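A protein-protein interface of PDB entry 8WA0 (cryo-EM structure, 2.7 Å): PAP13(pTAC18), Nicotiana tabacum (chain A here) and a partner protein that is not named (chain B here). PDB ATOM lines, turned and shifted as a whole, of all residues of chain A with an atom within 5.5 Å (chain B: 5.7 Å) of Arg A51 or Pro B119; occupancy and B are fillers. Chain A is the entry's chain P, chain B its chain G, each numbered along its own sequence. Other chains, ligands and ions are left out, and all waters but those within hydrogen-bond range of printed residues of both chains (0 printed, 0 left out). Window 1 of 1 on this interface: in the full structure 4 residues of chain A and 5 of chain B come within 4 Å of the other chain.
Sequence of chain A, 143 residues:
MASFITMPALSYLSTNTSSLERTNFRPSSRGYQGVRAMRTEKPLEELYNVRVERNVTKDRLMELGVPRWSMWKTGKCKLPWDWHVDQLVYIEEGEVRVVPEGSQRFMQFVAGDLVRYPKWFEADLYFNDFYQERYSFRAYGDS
The side-chain amide oxygen of Gln B92 sits close to the backbone carbonyl oxygen of Pro B119 (3.2 Å).
OD2 of Asp A86 lies within salt-bridge range of NE of Arg A116 (3.5 Å).
N of Arg A116 lies within hydrogen-bond range of O of Arg A51.
Leu B118 touches Asn A49 (CD2 to ND2, 3.6 Å).
CD of Pro B119 touches NH1 of Arg A51, 3.5 Å away.
OD2 of Asp A86 touches OD1 of Asn B116 (3.9 Å).
Printed residues of chain B within 4 Å of Arg A51: Pro B119 (3.5 Å).
Pro B119 touches just one residue of chain A: Arg A51 (3.5 Å).
Of the printed residues of chain A, Asn B116 touches Asp A86.
Of the printed residues of chain B, Asn A49 touches Leu B118.
Of the printed residues of chain A, Leu B118 touches Asn A49.
Of the printed residues of chain B, Asp A86 touches Asn B116 (3.9 Å).
Gln B92 touches none of the printed residues of chain A.
The nearest residue of chain B that does not touch Arg A51 is Leu B118 (4.1 Å).
Printed residues of chain A that touch a printed residue of chain B: Asn A49, Arg A51 and Asp A86.
Of the 8 printed residues of chain B, 3 touch a printed residue of chain A.
Hydrophobic or aromatic side chains of chain B within 4 Å of the printed part of chain A: Leu B118 and Pro B119.
Along chain B the printed residues that touch a printed residue of chain A span positions 116 to 119.
Among the printed residues, 3 pairs touch across the chains.
Among the printed residues, no Asp or Glu carboxylate lies within 4 Å of a Lys or Arg side-chain nitrogen of the other chain.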
ATOM      1  N   ASN A  49      36.827  -6.970 -10.604  1.00  0.00           N
ATOM      2  CA  ASN A  49      35.609  -7.771 -10.816  1.00  0.00           C
ATOM      3  C   ASN A  49      35.725  -9.063 -11.583  1.00  0.00           C
ATOM      4  O   ASN A  49      34.862  -9.380 -12.394  1.00  0.00           O
ATOM      5  CB  ASN A  49      34.444  -6.936 -11.346  1.00  0.00           C
ATOM      6  CG  ASN A  49      33.440  -6.608 -10.264  1.00  0.00           C
ATOM      7  OD1 ASN A  49      33.161  -7.433  -9.395  1.00  0.00           O
ATOM      8  ND2 ASN A  49      32.893  -5.402 -10.310  1.00  0.00           N
ATOM      9  N   VAL A  50      36.788  -9.813 -11.345  1.00  0.00           N
ATOM     10  CA  VAL A  50      36.873 -11.127 -11.946  1.00  0.00           C
ATOM     11  C   VAL A  50      36.406 -12.012 -10.816  1.00  0.00           C
ATOM     12  O   VAL A  50      37.112 -12.185  -9.828  1.00  0.00           O
ATOM     13  CB  VAL A  50      38.314 -11.493 -12.286  1.00  0.00           C
ATOM     14  N   ARG A  51      35.216 -12.573 -10.943  1.00  0.00           N
ATOM     15  CA  ARG A  51      34.675 -13.381  -9.873  1.00  0.00           C
ATOM     16  C   ARG A  51      35.130 -14.800 -10.112  1.00  0.00           C
ATOM     17  O   ARG A  51      35.069 -15.279 -11.243  1.00  0.00           O
ATOM     18  CB  ARG A  51      33.159 -13.316  -9.903  1.00  0.00           C
ATOM     19  CG  ARG A  51      32.613 -11.999 -10.421  1.00  0.00           C
ATOM     20  CD  ARG A  51      31.182 -12.164 -10.899  1.00  0.00           C
ATOM     21  NE  ARG A  51      30.782 -11.079 -11.787  1.00  0.00           N
ATOM     22  CZ  ARG A  51      29.651 -11.065 -12.482  1.00  0.00           C
ATOM     23  NH1 ARG A  51      28.804 -12.079 -12.397  1.00  0.00           N
ATOM     24  NH2 ARG A  51      29.369 -10.037 -13.268  1.00  0.00           N
ATOM     25  N   VAL A  52      35.585 -15.488  -9.070  1.00  0.00           N
ATOM     26  CA  VAL A  52      36.106 -16.812  -9.283  1.00  0.00           C
ATOM     27  C   VAL A  52      35.476 -17.769  -8.317  1.00  0.00           C
ATOM     28  O   VAL A  52      34.943 -17.338  -7.294  1.00  0.00           O
ATOM     29  CB  VAL A  52      37.604 -16.811  -9.018  1.00  0.00           C
ATOM     30  CG1 VAL A  52      37.927 -16.672  -7.542  1.00  0.00           C
ATOM     31  CG2 VAL A  52      38.289 -18.028  -9.619  1.00  0.00           C
ATOM     32  N   GLU A  53      35.443 -19.064  -8.627  1.00  0.00           N
ATOM     33  CA  GLU A  53      34.965 -20.061  -7.662  1.00  0.00           C
ATOM     34  C   GLU A  53      36.115 -20.997  -7.495  1.00  0.00           C
ATOM     35  O   GLU A  53      36.619 -21.507  -8.481  1.00  0.00           O
ATOM     36  CB  GLU A  53      33.765 -20.802  -8.190  1.00  0.00           C
ATOM     37  N   ASP A  86      31.737 -11.544 -21.956  1.00  0.00           N
ATOM     38  CA  ASP A  86      32.202 -12.331 -20.823  1.00  0.00           C
ATOM     39  C   ASP A  86      32.540 -13.781 -21.115  1.00  0.00           C
ATOM     40  O   ASP A  86      31.870 -14.413 -21.920  1.00  0.00           O
ATOM     41  CB  ASP A  86      31.178 -12.301 -19.726  1.00  0.00           C
ATOM     42  CG  ASP A  86      31.051 -10.938 -19.078  1.00  0.00           C
ATOM     43  OD1 ASP A  86      30.713  -9.968 -19.784  1.00  0.00           O
ATOM     44  OD2 ASP A  86      31.273 -10.841 -17.853  1.00  0.00           O
ATOM     45  N   LEU A 114      36.827 -21.655 -11.795  1.00  0.00           N
ATOM     46  CA  LEU A 114      36.011 -21.149 -12.881  1.00  0.00           C
ATOM     47  C   LEU A 114      36.027 -19.630 -12.781  1.00  0.00           C
ATOM     48  O   LEU A 114      35.540 -19.071 -11.804  1.00  0.00           O
ATOM     49  CB  LEU A 114      34.594 -21.687 -12.762  1.00  0.00           C
ATOM     50  CG  LEU A 114      33.549 -21.183 -13.758  1.00  0.00           C
ATOM     51  CD1 LEU A 114      33.821 -21.738 -15.143  1.00  0.00           C
ATOM     52  CD2 LEU A 114      32.158 -21.583 -13.298  1.00  0.00           C
ATOM     53  N   VAL A 115      36.609 -18.954 -13.767  1.00  0.00           N
ATOM     54  CA  VAL A 115      36.712 -17.501 -13.687  1.00  0.00           C
ATOM     55  C   VAL A 115      35.848 -16.761 -14.687  1.00  0.00           C
ATOM     56  O   VAL A 115      35.940 -17.050 -15.867  1.00  0.00           O
ATOM     57  CB  VAL A 115      38.130 -17.116 -14.073  1.00  0.00           C
ATOM     58  CG1 VAL A 115      38.421 -15.680 -13.668  1.00  0.00           C
ATOM     59  CG2 VAL A 115      39.139 -18.059 -13.445  1.00  0.00           C
ATOM     60  N   ARG A 116      35.035 -15.794 -14.278  1.00  0.00           N
ATOM     61  CA  ARG A 116      34.286 -15.033 -15.281  1.00  0.00           C
ATOM     62  C   ARG A 116      34.929 -13.713 -15.563  1.00  0.00           C
ATOM     63  O   ARG A 116      34.775 -12.776 -14.790  1.00  0.00           O
ATOM     64  CB  ARG A 116      32.876 -14.778 -14.806  1.00  0.00           C
ATOM     65  CG  ARG A 116      31.953 -14.163 -15.842  1.00  0.00           C
ATOM     66  CD  ARG A 116      30.537 -14.103 -15.304  1.00  0.00           C
ATOM     67  NE  ARG A 116      29.621 -13.437 -16.218  1.00  0.00           N
ATOM     68  CZ  ARG A 116      28.840 -14.067 -17.084  1.00  0.00           C
ATOM     69  NH1 ARG A 116      28.857 -15.391 -17.158  1.00  0.00           N
ATOM     70  NH2 ARG A 116      28.037 -13.375 -17.878  1.00  0.00           N
ATOM     71  N   GLN B  92      20.728 -13.437  -1.290  1.00  0.00           N
ATOM     72  CA  GLN B  92      21.828 -13.168  -2.146  1.00  0.00           C
ATOM     73  C   GLN B  92      22.837 -12.462  -1.279  1.00  0.00           C
ATOM     74  O   GLN B  92      24.034 -12.703  -1.395  1.00  0.00           O
ATOM     75  CB  GLN B  92      21.409 -12.326  -3.317  1.00  0.00           C
ATOM     76  CG  GLN B  92      22.219 -12.559  -4.571  1.00  0.00           C
ATOM     77  CD  GLN B  92      21.513 -12.046  -5.807  1.00  0.00           C
ATOM     78  OE1 GLN B  92      22.022 -12.165  -6.921  1.00  0.00           O
ATOM     79  NE2 GLN B  92      20.331 -11.473  -5.618  1.00  0.00           N
ATOM     80  N   ASN B 116      27.486  -3.233 -16.632  1.00  0.00           N
ATOM     81  CA  ASN B 116      27.546  -4.677 -16.601  1.00  0.00           C
ATOM     82  C   ASN B 116      27.015  -5.105 -15.295  1.00  0.00           C
ATOM     83  O   ASN B 116      27.752  -5.548 -14.442  1.00  0.00           O
ATOM     84  CB  ASN B 116      28.958  -5.186 -16.747  1.00  0.00           C
ATOM     85  CG  ASN B 116      29.012  -6.646 -17.152  1.00  0.00           C
ATOM     86  OD1 ASN B 116      29.916  -7.382 -16.757  1.00  0.00           O
ATOM     87  ND2 ASN B 116      28.032  -7.076 -17.938  1.00  0.00           N
ATOM     88  N   PRO B 117      25.715  -5.047 -15.162  1.00  0.00           N
ATOM     89  CA  PRO B 117      25.269  -5.351 -13.845  1.00  0.00           C
ATOM     90  C   PRO B 117      25.728  -6.618 -13.234  1.00  0.00           C
ATOM     91  O   PRO B 117      25.752  -7.655 -13.851  1.00  0.00           O
ATOM     92  CB  PRO B 117      23.790  -5.350 -14.017  1.00  0.00           C
ATOM     93  CG  PRO B 117      23.550  -4.238 -14.959  1.00  0.00           C
ATOM     94  CD  PRO B 117      24.667  -4.371 -15.940  1.00  0.00           C
ATOM     95  N   LEU B 118      26.091  -6.524 -11.987  1.00  0.00           N
ATOM     96  CA  LEU B 118      26.568  -7.622 -11.247  1.00  0.00           C
ATOM     97  C   LEU B 118      25.389  -8.440 -10.916  1.00  0.00           C
ATOM     98  O   LEU B 118      24.270  -8.010 -11.112  1.00  0.00           O
ATOM     99  CB  LEU B 118      27.185  -7.094  -9.965  1.00  0.00           C
ATOM    100  CG  LEU B 118      28.437  -6.221  -9.956  1.00  0.00           C
ATOM    101  CD1 LEU B 118      28.748  -5.783  -8.536  1.00  0.00           C
ATOM    102  CD2 LEU B 118      29.628  -6.938 -10.553  1.00  0.00           C
ATOM    103  N   PRO B 119      25.607  -9.670 -10.392  1.00  0.00           N
ATOM    104  CA  PRO B 119      24.432 -10.503 -10.211  1.00  0.00           C
ATOM    105  C   PRO B 119      23.342 -10.000  -9.325  1.00  0.00           C
ATOM    106  O   PRO B 119      22.200 -10.352  -9.560  1.00  0.00           O
ATOM    107  CB  PRO B 119      25.017 -11.758  -9.592  1.00  0.00           C
ATOM    108  CG  PRO B 119      26.300 -11.355  -8.979  1.00  0.00           C
ATOM    109  CD  PRO B 119      26.817 -10.444 -10.023  1.00  0.00           C
ATOM    110  N   GLU B 120      23.643  -9.184  -8.341  1.00  0.00           N
ATOM    111  CA  GLU B 120      22.654  -8.764  -7.389  1.00  0.00           C
ATOM    112  C   GLU B 120      21.886  -7.543  -7.737  1.00  0.00           C
ATOM    113  O   GLU B 120      21.091  -7.085  -6.945  1.00  0.00           O
ATOM    114  CB  GLU B 120      23.313  -8.561  -6.063  1.00  0.00           C
ATOM    115  CG  GLU B 120      24.283  -9.664  -5.686  1.00  0.00           C
ATOM    116  CD  GLU B 120      24.646  -9.634  -4.216  1.00  0.00           C
ATOM    117  OE1 GLU B 120      25.401 -10.523  -3.770  1.00  0.00           O
ATOM    118  OE2 GLU B 120      24.171  -8.723  -3.506  1.00  0.00           O
ATOM    119  N   PHE B 121      22.097  -6.950  -8.893  1.00  0.00           N
ATOM    120  CA  PHE B 121      21.447  -5.666  -9.182  1.00  0.00           C
ATOM    121  C   PHE B 121      19.940  -5.656  -9.150  1.00  0.00           C
ATOM    122  O   PHE B 121      19.288  -4.832  -8.436  1.00  0.00           O
ATOM    123  CB  PHE B 121      21.903  -5.194 -10.563  1.00  0.00           C
ATOM    124  CG  PHE B 121      21.305  -3.888 -10.999  1.00  0.00           C
ATOM    125  CD1 PHE B 121      21.735  -2.698 -10.448  1.00  0.00           C
ATOM    126  CD2 PHE B 121      20.336  -3.852 -11.985  1.00  0.00           C
ATOM    127  CE1 PHE B 121      21.194  -1.496 -10.856  1.00  0.00           C
ATOM    128  CE2 PHE B 121      19.791  -2.654 -12.395  1.00  0.00           C
ATOM    129  CZ  PHE B 121      20.221  -1.473 -11.831  1.00  0.00           C
ATOM    130  N   SER B 122      19.359  -6.625  -9.825  1.00  0.00           N
ATOM    131  CA  SER B 122      17.925  -6.588  -9.999  1.00  0.00           C
ATOM    132  C   SER B 122      17.101  -6.568  -8.762  1.00  0.00           C
ATOM    133  O   SER B 122      16.193  -5.751  -8.652  1.00  0.00           O
ATOM    134  CB  SER B 122      17.537  -7.815 -10.801  1.00  0.00           C
ATOM    135  OG  SER B 122      18.322  -7.906 -11.976  1.00  0.00           O
